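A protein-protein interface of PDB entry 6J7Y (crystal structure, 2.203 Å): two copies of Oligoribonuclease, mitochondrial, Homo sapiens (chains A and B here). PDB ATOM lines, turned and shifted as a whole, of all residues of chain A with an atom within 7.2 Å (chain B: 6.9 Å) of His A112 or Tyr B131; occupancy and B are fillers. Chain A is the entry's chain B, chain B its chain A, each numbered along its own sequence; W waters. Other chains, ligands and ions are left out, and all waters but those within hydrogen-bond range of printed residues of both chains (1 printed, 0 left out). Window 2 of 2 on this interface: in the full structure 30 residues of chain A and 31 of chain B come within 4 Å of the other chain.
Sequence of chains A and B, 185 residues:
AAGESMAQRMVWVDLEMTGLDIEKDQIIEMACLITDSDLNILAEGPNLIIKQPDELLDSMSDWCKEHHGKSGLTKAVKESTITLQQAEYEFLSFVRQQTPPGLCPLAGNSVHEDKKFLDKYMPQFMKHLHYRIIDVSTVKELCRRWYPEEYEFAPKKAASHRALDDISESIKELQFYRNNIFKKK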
ATOM      1  N   LEU A  20      35.967   2.664  38.166  1.00  0.00           N
ATOM      2  CA  LEU A  20      35.584   3.110  36.831  1.00  0.00           C
ATOM      3  C   LEU A  20      36.761   3.180  35.867  1.00  0.00           C
ATOM      4  O   LEU A  20      36.591   3.655  34.740  1.00  0.00           O
ATOM      5  CB  LEU A  20      34.883   4.466  36.903  1.00  0.00           C
ATOM      6  CG  LEU A  20      33.650   4.459  37.810  1.00  0.00           C
ATOM      7  CD1 LEU A  20      33.781   5.518  38.894  1.00  0.00           C
ATOM      8  CD2 LEU A  20      32.372   4.633  37.003  1.00  0.00           C
ATOM      9  N   LEU A 106      20.982  -2.954  24.716  1.00  0.00           N
ATOM     10  CA  LEU A 106      21.261  -2.877  26.141  1.00  0.00           C
ATOM     11  C   LEU A 106      20.457  -1.746  26.768  1.00  0.00           C
ATOM     12  O   LEU A 106      20.326  -0.672  26.185  1.00  0.00           O
ATOM     13  CB  LEU A 106      22.744  -2.616  26.352  1.00  0.00           C
ATOM     14  CG  LEU A 106      23.486  -3.045  27.592  1.00  0.00           C
ATOM     15  CD1 LEU A 106      23.275  -4.533  27.844  1.00  0.00           C
ATOM     16  CD2 LEU A 106      24.966  -2.728  27.361  1.00  0.00           C
ATOM     17  N   GLY A 108      19.444   0.253  30.738  1.00  0.00           N
ATOM     18  CA  GLY A 108      19.795   0.434  32.134  1.00  0.00           C
ATOM     19  C   GLY A 108      20.061   1.894  32.434  1.00  0.00           C
ATOM     20  O   GLY A 108      19.958   2.761  31.563  1.00  0.00           O
ATOM     21  N   ASN A 109      20.417   2.148  33.700  1.00  0.00           N
ATOM     22  CA  ASN A 109      20.678   3.514  34.158  1.00  0.00           C
ATOM     23  C   ASN A 109      22.098   3.956  33.816  1.00  0.00           C
ATOM     24  O   ASN A 109      22.300   5.024  33.230  1.00  0.00           O
ATOM     25  CB  ASN A 109      20.442   3.633  35.670  1.00  0.00           C
ATOM     26  CG  ASN A 109      19.080   4.219  36.006  1.00  0.00           C
ATOM     27  OD1 ASN A 109      18.255   3.544  36.602  1.00  0.00           O
ATOM     28  ND2 ASN A 109      18.841   5.483  35.623  1.00  0.00           N
ATOM     29  N   SER A 110      23.088   3.162  34.195  1.00  0.00           N
ATOM     30  CA  SER A 110      24.488   3.455  33.882  1.00  0.00           C
ATOM     31  C   SER A 110      24.934   2.655  32.671  1.00  0.00           C
ATOM     32  O   SER A 110      25.967   1.980  32.693  1.00  0.00           O
ATOM     33  CB  SER A 110      25.370   3.149  35.084  1.00  0.00           C
ATOM     34  OG  SER A 110      25.215   1.799  35.489  1.00  0.00           O
ATOM     35  N   VAL A 111      24.144   2.698  31.599  1.00  0.00           N
ATOM     36  CA  VAL A 111      24.318   1.645  30.617  1.00  0.00           C
ATOM     37  C   VAL A 111      25.507   1.918  29.703  1.00  0.00           C
ATOM     38  O   VAL A 111      26.155   0.970  29.254  1.00  0.00           O
ATOM     39  CB  VAL A 111      23.014   1.409  29.835  1.00  0.00           C
ATOM     40  CG1 VAL A 111      22.884   2.359  28.679  1.00  0.00           C
ATOM     41  CG2 VAL A 111      22.956  -0.019  29.362  1.00  0.00           C
ATOM     42  N   HIS A 112      25.857   3.187  29.436  1.00  0.00           N
ATOM     43  CA  HIS A 112      27.043   3.413  28.607  1.00  0.00           C
ATOM     44  C   HIS A 112      28.332   3.045  29.341  1.00  0.00           C
ATOM     45  O   HIS A 112      29.260   2.505  28.728  1.00  0.00           O
ATOM     46  CB  HIS A 112      27.094   4.857  28.091  1.00  0.00           C
ATOM     47  CG  HIS A 112      26.822   5.903  29.128  1.00  0.00           C
ATOM     48  ND1 HIS A 112      27.829   6.569  29.794  1.00  0.00           N
ATOM     49  CD2 HIS A 112      25.659   6.432  29.580  1.00  0.00           C
ATOM     50  CE1 HIS A 112      27.300   7.449  30.627  1.00  0.00           C
ATOM     51  NE2 HIS A 112      25.985   7.385  30.517  1.00  0.00           N
ATOM     52  N   GLU A 113      28.393   3.261  30.656  1.00  0.00           N
ATOM     53  CA  GLU A 113      29.542   2.784  31.425  1.00  0.00           C
ATOM     54  C   GLU A 113      29.605   1.257  31.432  1.00  0.00           C
ATOM     55  O   GLU A 113      30.667   0.655  31.192  1.00  0.00           O
ATOM     56  CB  GLU A 113      29.469   3.339  32.847  1.00  0.00           C
ATOM     57  CG  GLU A 113      30.762   3.206  33.659  1.00  0.00           C
ATOM     58  CD  GLU A 113      31.918   4.043  33.121  1.00  0.00           C
ATOM     59  OE1 GLU A 113      31.675   5.004  32.354  1.00  0.00           O
ATOM     60  OE2 GLU A 113      33.078   3.739  33.479  1.00  0.00           O
ATOM     61  N   ASP A 114      28.469   0.612  31.712  1.00  0.00           N
ATOM     62  CA  ASP A 114      28.421  -0.847  31.693  1.00  0.00           C
ATOM     63  C   ASP A 114      28.805  -1.389  30.324  1.00  0.00           C
ATOM     64  O   ASP A 114      29.515  -2.393  30.224  1.00  0.00           O
ATOM     65  CB  ASP A 114      27.027  -1.326  32.090  1.00  0.00           C
ATOM     66  CG  ASP A 114      26.779  -1.190  33.570  1.00  0.00           C
ATOM     67  OD1 ASP A 114      27.719  -0.810  34.293  1.00  0.00           O
ATOM     68  OD2 ASP A 114      25.660  -1.474  34.014  1.00  0.00           O
ATOM     69  N   LYS A 115      28.356  -0.727  29.260  1.00  0.00           N
ATOM     70  CA  LYS A 115      28.709  -1.166  27.917  1.00  0.00           C
ATOM     71  C   LYS A 115      30.198  -1.009  27.671  1.00  0.00           C
ATOM     72  O   LYS A 115      30.811  -1.846  27.002  1.00  0.00           O
ATOM     73  CB  LYS A 115      27.919  -0.380  26.880  1.00  0.00           C
ATOM     74  CG  LYS A 115      28.310  -0.691  25.451  1.00  0.00           C
ATOM     75  CD  LYS A 115      27.364  -0.005  24.490  1.00  0.00           C
ATOM     76  CE  LYS A 115      27.719  -0.329  23.057  1.00  0.00           C
ATOM     77  NZ  LYS A 115      29.024   0.289  22.716  1.00  0.00           N
ATOM     78  N   LYS A 116      30.797   0.056  28.206  1.00  0.00           N
ATOM     79  CA  LYS A 116      32.248   0.181  28.135  1.00  0.00           C
ATOM     80  C   LYS A 116      32.918  -1.054  28.725  1.00  0.00           C
ATOM     81  O   LYS A 116      33.795  -1.659  28.100  1.00  0.00           O
ATOM     82  CB  LYS A 116      32.703   1.457  28.852  1.00  0.00           C
ATOM     83  CG  LYS A 116      34.202   1.539  29.116  1.00  0.00           C
ATOM     84  CD  LYS A 116      34.673   2.991  29.261  1.00  0.00           C
ATOM     85  CE  LYS A 116      34.098   3.657  30.498  1.00  0.00           C
ATOM     86  NZ  LYS A 116      34.104   5.145  30.385  1.00  0.00           N
ATOM     87  N   PHE A 117      32.469  -1.481  29.907  1.00  0.00           N
ATOM     88  CA  PHE A 117      33.124  -2.630  30.541  1.00  0.00           C
ATOM     89  C   PHE A 117      32.804  -3.950  29.846  1.00  0.00           C
ATOM     90  O   PHE A 117      33.635  -4.871  29.845  1.00  0.00           O
ATOM     91  CB  PHE A 117      32.752  -2.713  32.015  1.00  0.00           C
ATOM     92  CG  PHE A 117      33.690  -1.955  32.896  1.00  0.00           C
ATOM     93  CD1 PHE A 117      33.503  -0.596  33.122  1.00  0.00           C
ATOM     94  CD2 PHE A 117      34.787  -2.589  33.464  1.00  0.00           C
ATOM     95  CE1 PHE A 117      34.385   0.114  33.924  1.00  0.00           C
ATOM     96  CE2 PHE A 117      35.665  -1.891  34.264  1.00  0.00           C
ATOM     97  CZ  PHE A 117      35.466  -0.533  34.494  1.00  0.00           C
ATOM     98  N   LEU A 118      31.622  -4.058  29.240  1.00  0.00           N
ATOM     99  CA  LEU A 118      31.222  -5.297  28.579  1.00  0.00           C
ATOM    100  C   LEU A 118      31.894  -5.453  27.218  1.00  0.00           C
ATOM    101  O   LEU A 118      32.274  -6.566  26.838  1.00  0.00           O
ATOM    102  CB  LEU A 118      29.697  -5.341  28.424  1.00  0.00           C
ATOM    103  CG  LEU A 118      28.909  -5.458  29.730  1.00  0.00           C
ATOM    104  CD1 LEU A 118      27.437  -5.168  29.490  1.00  0.00           C
ATOM    105  CD2 LEU A 118      29.103  -6.856  30.352  1.00  0.00           C
ATOM    106  N   ASP A 119      32.021  -4.357  26.465  1.00  0.00           N
ATOM    107  CA  ASP A 119      32.754  -4.401  25.204  1.00  0.00           C
ATOM    108  C   ASP A 119      34.160  -4.938  25.410  1.00  0.00           C
ATOM    109  O   ASP A 119      34.669  -5.706  24.587  1.00  0.00           O
ATOM    110  CB  ASP A 119      32.817  -3.009  24.580  1.00  0.00           C
ATOM    111  CG  ASP A 119      31.531  -2.619  23.907  1.00  0.00           C
ATOM    112  OD1 ASP A 119      30.806  -3.530  23.447  1.00  0.00           O
ATOM    113  OD2 ASP A 119      31.250  -1.403  23.839  1.00  0.00           O
ATOM    114  N   ILE A 133      21.604   1.817  22.550  1.00  0.00           N
ATOM    115  CA  ILE A 133      21.354   1.659  23.970  1.00  0.00           C
ATOM    116  C   ILE A 133      20.078   2.398  24.343  1.00  0.00           C
ATOM    117  O   ILE A 133      19.665   3.368  23.699  1.00  0.00           O
ATOM    118  CB  ILE A 133      22.532   2.170  24.828  1.00  0.00           C
ATOM    119  CG1 ILE A 133      22.651   3.693  24.683  1.00  0.00           C
ATOM    120  CG2 ILE A 133      23.832   1.441  24.439  1.00  0.00           C
ATOM    121  CD1 ILE A 133      23.380   4.385  25.821  1.00  0.00           C
ATOM    122  N   ILE A 134      19.461   1.937  25.422  1.00  0.00           N
ATOM    123  CA  ILE A 134      18.359   2.635  26.056  1.00  0.00           C
ATOM    124  C   ILE A 134      18.864   3.080  27.418  1.00  0.00           C
ATOM    125  O   ILE A 134      18.889   2.287  28.368  1.00  0.00           O
ATOM    126  CB  ILE A 134      17.120   1.755  26.193  1.00  0.00           C
ATOM    127  CG1 ILE A 134      16.640   1.301  24.820  1.00  0.00           C
ATOM    128  CG2 ILE A 134      16.053   2.508  27.003  1.00  0.00           C
ATOM    129  CD1 ILE A 134      15.953   2.350  24.068  1.00  0.00           C
ATOM    130  N   ASP A 135      19.220   4.356  27.512  1.00  0.00           N
ATOM    131  CA  ASP A 135      19.862   4.947  28.681  1.00  0.00           C
ATOM    132  C   ASP A 135      18.790   5.651  29.499  1.00  0.00           C
ATOM    133  O   ASP A 135      18.327   6.732  29.135  1.00  0.00           O
ATOM    134  CB  ASP A 135      20.962   5.910  28.239  1.00  0.00           C
ATOM    135  CG  ASP A 135      21.590   6.670  29.398  1.00  0.00           C
ATOM    136  OD1 ASP A 135      21.429   6.264  30.570  1.00  0.00           O
ATOM    137  OD2 ASP A 135      22.240   7.698  29.126  1.00  0.00           O
ATOM    138  N   SER A 137      19.148   7.138  32.185  1.00  0.00           N
ATOM    139  CA  SER A 137      19.668   8.379  32.752  1.00  0.00           C
ATOM    140  C   SER A 137      19.493   9.563  31.807  1.00  0.00           C
ATOM    141  O   SER A 137      19.345  10.696  32.271  1.00  0.00           O
ATOM    142  CB  SER A 137      21.135   8.203  33.134  1.00  0.00           C
ATOM    143  OG  SER A 137      21.214   7.750  34.476  1.00  0.00           O
ATOM    144  N   THR A 138      19.485   9.326  30.491  1.00  0.00           N
ATOM    145  CA  THR A 138      19.085  10.378  29.551  1.00  0.00           C
ATOM    146  C   THR A 138      17.669  10.868  29.845  1.00  0.00           C
ATOM    147  O   THR A 138      17.400  12.078  29.877  1.00  0.00           O
ATOM    148  CB  THR A 138      19.161   9.853  28.119  1.00  0.00           C
ATOM    149  OG1 THR A 138      20.526   9.734  27.723  1.00  0.00           O
ATOM    150  CG2 THR A 138      18.401  10.776  27.169  1.00  0.00           C
ATOM    151  N   GLY B 102      31.815  20.296  36.022  1.00  0.00           N
ATOM    152  CA  GLY B 102      31.261  19.002  36.362  1.00  0.00           C
ATOM    153  C   GLY B 102      29.752  18.878  36.291  1.00  0.00           C
ATOM    154  O   GLY B 102      29.234  17.788  36.534  1.00  0.00           O
ATOM    155  N   LEU B 103      29.021  19.934  35.936  1.00  0.00           N
ATOM    156  CA  LEU B 103      27.568  19.885  36.057  1.00  0.00           C
ATOM    157  C   LEU B 103      26.839  19.616  34.745  1.00  0.00           C
ATOM    158  O   LEU B 103      25.700  19.129  34.783  1.00  0.00           O
ATOM    159  CB  LEU B 103      27.042  21.199  36.671  1.00  0.00           C
ATOM    160  CG  LEU B 103      27.551  21.580  38.076  1.00  0.00           C
ATOM    161  CD1 LEU B 103      26.785  22.783  38.637  1.00  0.00           C
ATOM    162  CD2 LEU B 103      27.457  20.396  39.039  1.00  0.00           C
ATOM    163  N   CYS B 104      27.455  19.887  33.581  1.00  0.00           N
ATOM    164  CA  CYS B 104      26.572  19.745  32.412  1.00  0.00           C
ATOM    165  C   CYS B 104      26.926  18.528  31.555  1.00  0.00           C
ATOM    166  O   CYS B 104      28.103  18.160  31.438  1.00  0.00           O
ATOM    167  CB  CYS B 104      26.621  21.014  31.555  1.00  0.00           C
ATOM    168  SG  CYS B 104      26.013  22.493  32.496  1.00  0.00           S
ATOM    169  N   PRO B 105      25.930  17.878  30.957  1.00  0.00           N
ATOM    170  CA  PRO B 105      26.187  16.656  30.196  1.00  0.00           C
ATOM    171  C   PRO B 105      26.511  16.885  28.727  1.00  0.00           C
ATOM    172  O   PRO B 105      26.032  17.821  28.086  1.00  0.00           O
ATOM    173  CB  PRO B 105      24.852  15.911  30.320  1.00  0.00           C
ATOM    174  CG  PRO B 105      23.835  17.050  30.336  1.00  0.00           C
ATOM    175  CD  PRO B 105      24.483  18.154  31.094  1.00  0.00           C
ATOM    176  N   LEU B 106      27.301  15.955  28.191  1.00  0.00           N
ATOM    177  CA  LEU B 106      27.407  15.792  26.744  1.00  0.00           C
ATOM    178  C   LEU B 106      26.063  15.403  26.134  1.00  0.00           C
ATOM    179  O   LEU B 106      25.335  14.574  26.685  1.00  0.00           O
ATOM    180  CB  LEU B 106      28.431  14.706  26.430  1.00  0.00           C
ATOM    181  CG  LEU B 106      29.431  14.896  25.303  1.00  0.00           C
ATOM    182  CD1 LEU B 106      30.002  16.307  25.332  1.00  0.00           C
ATOM    183  CD2 LEU B 106      30.536  13.833  25.426  1.00  0.00           C
ATOM    184  N   HIS B 112      27.260   8.344  23.294  1.00  0.00           N
ATOM    185  CA  HIS B 112      28.085   7.449  24.105  1.00  0.00           C
ATOM    186  C   HIS B 112      29.348   7.012  23.355  1.00  0.00           C
ATOM    187  O   HIS B 112      30.416   6.877  23.967  1.00  0.00           O
ATOM    188  CB  HIS B 112      27.266   6.254  24.616  1.00  0.00           C
ATOM    189  CG  HIS B 112      26.691   5.382  23.546  1.00  0.00           C
ATOM    190  ND1 HIS B 112      27.318   4.237  23.105  1.00  0.00           N
ATOM    191  CD2 HIS B 112      25.527   5.465  22.857  1.00  0.00           C
ATOM    192  CE1 HIS B 112      26.575   3.661  22.175  1.00  0.00           C
ATOM    193  NE2 HIS B 112      25.485   4.387  22.006  1.00  0.00           N
ATOM    194  N   GLU B 113      29.284   6.900  22.027  1.00  0.00           N
ATOM    195  CA  GLU B 113      30.493   6.591  21.261  1.00  0.00           C
ATOM    196  C   GLU B 113      31.478   7.762  21.257  1.00  0.00           C
ATOM    197  O   GLU B 113      32.692   7.572  21.443  1.00  0.00           O
ATOM    198  CB  GLU B 113      30.109   6.195  19.835  1.00  0.00           C
ATOM    199  CG  GLU B 113      29.537   4.778  19.711  1.00  0.00           C
ATOM    200  CD  GLU B 113      30.611   3.681  19.777  1.00  0.00           C
ATOM    201  OE1 GLU B 113      30.926   3.090  18.717  1.00  0.00           O
ATOM    202  OE2 GLU B 113      31.124   3.396  20.886  1.00  0.00           O
ATOM    203  N   LYS B 115      31.668  10.079  23.523  1.00  0.00           N
ATOM    204  CA  LYS B 115      32.178  10.141  24.886  1.00  0.00           C
ATOM    205  C   LYS B 115      33.256   9.090  25.109  1.00  0.00           C
ATOM    206  O   LYS B 115      34.263   9.361  25.771  1.00  0.00           O
ATOM    207  CB  LYS B 115      31.048   9.949  25.899  1.00  0.00           C
ATOM    208  CG  LYS B 115      31.534  10.160  27.324  1.00  0.00           C
ATOM    209  CD  LYS B 115      30.449   9.983  28.356  1.00  0.00           C
ATOM    210  CE  LYS B 115      30.972  10.307  29.759  1.00  0.00           C
ATOM    211  NZ  LYS B 115      31.202   9.074  30.571  1.00  0.00           N
ATOM    212  N   LYS B 116      33.068   7.887  24.558  1.00  0.00           N
ATOM    213  CA  LYS B 116      34.115   6.878  24.639  1.00  0.00           C
ATOM    214  C   LYS B 116      35.409   7.408  24.038  1.00  0.00           C
ATOM    215  O   LYS B 116      36.489   7.260  24.621  1.00  0.00           O
ATOM    216  CB  LYS B 116      33.670   5.593  23.936  1.00  0.00           C
ATOM    217  CG  LYS B 116      34.777   4.553  23.797  1.00  0.00           C
ATOM    218  CD  LYS B 116      34.284   3.157  24.148  1.00  0.00           C
ATOM    219  CE  LYS B 116      33.742   2.427  22.929  1.00  0.00           C
ATOM    220  NZ  LYS B 116      33.358   1.020  23.261  1.00  0.00           N
ATOM    221  N   ASP B 119      36.763  10.592  26.356  1.00  0.00           N
ATOM    222  CA  ASP B 119      37.269  10.180  27.659  1.00  0.00           C
ATOM    223  C   ASP B 119      38.737   9.790  27.576  1.00  0.00           C
ATOM    224  O   ASP B 119      39.477   9.928  28.551  1.00  0.00           O
ATOM    225  CB  ASP B 119      36.435   9.006  28.197  1.00  0.00           C
ATOM    226  CG  ASP B 119      35.122   9.449  28.849  1.00  0.00           C
ATOM    227  OD1 ASP B 119      34.899  10.671  29.034  1.00  0.00           O
ATOM    228  OD2 ASP B 119      34.302   8.567  29.182  1.00  0.00           O
ATOM    229  N   MET B 126      36.624  16.330  29.079  1.00  0.00           N
ATOM    230  CA  MET B 126      35.516  15.558  29.654  1.00  0.00           C
ATOM    231  C   MET B 126      35.422  15.718  31.168  1.00  0.00           C
ATOM    232  O   MET B 126      34.335  15.604  31.744  1.00  0.00           O
ATOM    233  CB  MET B 126      35.665  14.076  29.307  1.00  0.00           C
ATOM    234  CG  MET B 126      35.503  13.799  27.833  1.00  0.00           C
ATOM    235  SD  MET B 126      33.883  14.381  27.318  1.00  0.00           S
ATOM    236  CE  MET B 126      32.805  13.473  28.403  1.00  0.00           C
ATOM    237  N   LEU B 129      32.877  18.103  32.299  1.00  0.00           N
ATOM    238  CA  LEU B 129      31.481  17.756  32.072  1.00  0.00           C
ATOM    239  C   LEU B 129      30.956  16.783  33.123  1.00  0.00           C
ATOM    240  O   LEU B 129      31.712  16.090  33.797  1.00  0.00           O
ATOM    241  CB  LEU B 129      31.303  17.141  30.679  1.00  0.00           C
ATOM    242  CG  LEU B 129      31.874  18.049  29.591  1.00  0.00           C
ATOM    243  CD1 LEU B 129      31.717  17.432  28.196  1.00  0.00           C
ATOM    244  CD2 LEU B 129      31.204  19.405  29.684  1.00  0.00           C
ATOM    245  N   HIS B 130      29.634  16.715  33.229  1.00  0.00           N
ATOM    246  CA  HIS B 130      29.020  15.651  34.008  1.00  0.00           C
ATOM    247  C   HIS B 130      29.399  14.291  33.406  1.00  0.00           C
ATOM    248  O   HIS B 130      29.931  14.199  32.300  1.00  0.00           O
ATOM    249  CB  HIS B 130      27.505  15.834  34.023  1.00  0.00           C
ATOM    250  CG  HIS B 130      26.822  15.247  35.222  1.00  0.00           C
ATOM    251  ND1 HIS B 130      26.286  13.976  35.227  1.00  0.00           N
ATOM    252  CD2 HIS B 130      26.559  15.770  36.443  1.00  0.00           C
ATOM    253  CE1 HIS B 130      25.726  13.742  36.399  1.00  0.00           C
ATOM    254  NE2 HIS B 130      25.878  14.815  37.155  1.00  0.00           N
ATOM    255  N   TYR B 131      29.116  13.221  34.144  1.00  0.00           N
ATOM    256  CA  TYR B 131      29.346  11.893  33.593  1.00  0.00           C
ATOM    257  C   TYR B 131      28.108  11.358  32.881  1.00  0.00           C
ATOM    258  O   TYR B 131      28.239  10.563  31.944  1.00  0.00           O
ATOM    259  CB  TYR B 131      29.819  10.923  34.702  1.00  0.00           C
ATOM    260  CG  TYR B 131      28.810  10.706  35.809  1.00  0.00           C
ATOM    261  CD1 TYR B 131      27.769   9.793  35.665  1.00  0.00           C
ATOM    262  CD2 TYR B 131      28.886  11.434  36.997  1.00  0.00           C
ATOM    263  CE1 TYR B 131      26.827   9.613  36.680  1.00  0.00           C
ATOM    264  CE2 TYR B 131      27.960  11.251  38.015  1.00  0.00           C
ATOM    265  CZ  TYR B 131      26.938  10.342  37.849  1.00  0.00           C
ATOM    266  OH  TYR B 131      26.018  10.168  38.852  1.00  0.00           O
ATOM    267  N   ARG B 132      26.908  11.798  33.273  1.00  0.00           N
ATOM    268  CA  ARG B 132      25.713  11.452  32.501  1.00  0.00           C
ATOM    269  C   ARG B 132      25.760  12.087  31.110  1.00  0.00           C
ATOM    270  O   ARG B 132      26.498  13.039  30.853  1.00  0.00           O
ATOM    271  CB  ARG B 132      24.437  11.899  33.222  1.00  0.00           C
ATOM    272  CG  ARG B 132      24.209  11.203  34.562  1.00  0.00           C
ATOM    273  CD  ARG B 132      22.869  11.587  35.157  1.00  0.00           C
ATOM    274  NE  ARG B 132      22.617  10.870  36.396  1.00  0.00           N
ATOM    275  CZ  ARG B 132      22.296  11.443  37.550  1.00  0.00           C
ATOM    276  NH1 ARG B 132      22.153  12.762  37.631  1.00  0.00           N
ATOM    277  NH2 ARG B 132      22.094  10.690  38.626  1.00  0.00           N
ATOM    278  N   ILE B 133      24.950  11.544  30.203  1.00  0.00           N
ATOM    279  CA  ILE B 133      24.843  12.056  28.846  1.00  0.00           C
ATOM    280  C   ILE B 133      23.372  12.227  28.532  1.00  0.00           C
ATOM    281  O   ILE B 133      22.497  11.682  29.205  1.00  0.00           O
ATOM    282  CB  ILE B 133      25.476  11.141  27.775  1.00  0.00           C
ATOM    283  CG1 ILE B 133      24.721   9.813  27.723  1.00  0.00           C
ATOM    284  CG2 ILE B 133      26.965  10.936  28.024  1.00  0.00           C
ATOM    285  CD1 ILE B 133      25.387   8.764  26.864  1.00  0.00           C
ATOM    286  N   ASP B 135      21.397  11.234  25.448  1.00  0.00           N
ATOM    287  CA  ASP B 135      21.560  10.398  24.272  1.00  0.00           C
ATOM    288  C   ASP B 135      20.251  10.501  23.512  1.00  0.00           C
ATOM    289  O   ASP B 135      19.253   9.878  23.895  1.00  0.00           O
ATOM    290  CB  ASP B 135      21.889   8.971  24.692  1.00  0.00           C
ATOM    291  CG  ASP B 135      21.992   8.024  23.526  1.00  0.00           C
ATOM    292  OD1 ASP B 135      22.222   8.490  22.385  1.00  0.00           O
ATOM    293  OD2 ASP B 135      21.840   6.805  23.765  1.00  0.00           O
HETATM  294  O   HOH W   1      23.518   9.200  30.878  1.00  0.00           O
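OD2 of Asp B119 is in salt-bridge range of NZ of Lys A116. The side-chain hydroxyl (OG1) of Thr A138 sits at hydrogen-bond distance from the backbone NH (N) of Asp B135 (2.9 Å). The side-chain carboxylate (OD2) of Asp A119 is in salt-bridge range of the side-chain amino group (NZ) of Lys B116 (3.3 Å). The side-chain hydroxyl (OG1) of Thr A138 sits at hydrogen-bond distance from the backbone carbonyl oxygen (O) of Ile B133.
Water W1 lies within hydrogen-bond range of OD2 of Asp A135 (2.6 Å), N of Ile B133 (2.8 Å) and NE2 of His A112 (3.1 Å).
The side-chain hydroxyl (OG) of Ser A137 sits at hydrogen-bond distance from the backbone carbonyl oxygen (O) of Asn A109, at 3.2 Å. N of Arg B132 is in hydrogen-bond range of ND1 of His B130. The side-chain amino group (NZ) of Lys B115 is in salt-bridge range of the side-chain carboxylate (OD2) of Asp B119 (3.4 Å). The side-chain hydroxyl of Thr A138 is in hydrogen-bond range of the side-chain carboxylate of Asp A135. The side-chain carboxylate (OD1) of Asp A135 is in hydrogen-bond range of the backbone NH (N) of Ser A137, 2.9 Å away. The side-chain amino group (NZ) of Lys A116 is in salt-bridge range of the side-chain carboxylate (OE1) of Glu A113, at 3.1 Å.
Of the 17 printed residues of chain B, 7 touch a printed residue of chain A. Printed residues of chain B that touch a printed residue of chain A: His B112, Lys B116, Asp B119, Tyr B131, Arg B132, Ile B133 and Asp B135. Of the 19 printed residues of chain A, 7 touch a printed residue of chain B.
His A112 touches its own counterpart, His B112. His A112 touches Ile B133, and with the chains exchanged Ile A133 touches His B112. Lys A116 touches Asp B119, and with the chains exchanged Asp A119 touches Lys B116. Ile A133 touches Asp B135, and with the chains exchanged Asp A135 touches Ile B133. Of the 11 pairs that touch across the chains among the printed residues, 7 have their exchanged pair printed and touching as well.
Among the printed residues, merely in contact across the chains: Ile A133 with Asp B135, His A112 with Tyr B131, Asp A135 with Ile B133, His A112 with Ile B133, His A112 with His B112, Ile A133 with His B112 and Ser A137 with Arg B132.
His A112 touches just these residues of chain B: His B112, Tyr B131 and Ile B133. Of chain A, only His A112 (3.5 Å) comes within 4 Å of Tyr B131. Of the printed residues of chain B, Thr A138 touches Ile B133 (3.1 Å) and Asp B135 (2.9 Å). Printed residues of chain A within 4 Å of Asp B119: Lys A116 (3.6 Å). Printed residues of chain B within 4 Å of Ile A133: His B112 and Asp B135. Of the printed residues of chain B, Ser A137 touches Arg B132. Met B126 touches none of the printed residues of chain A.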
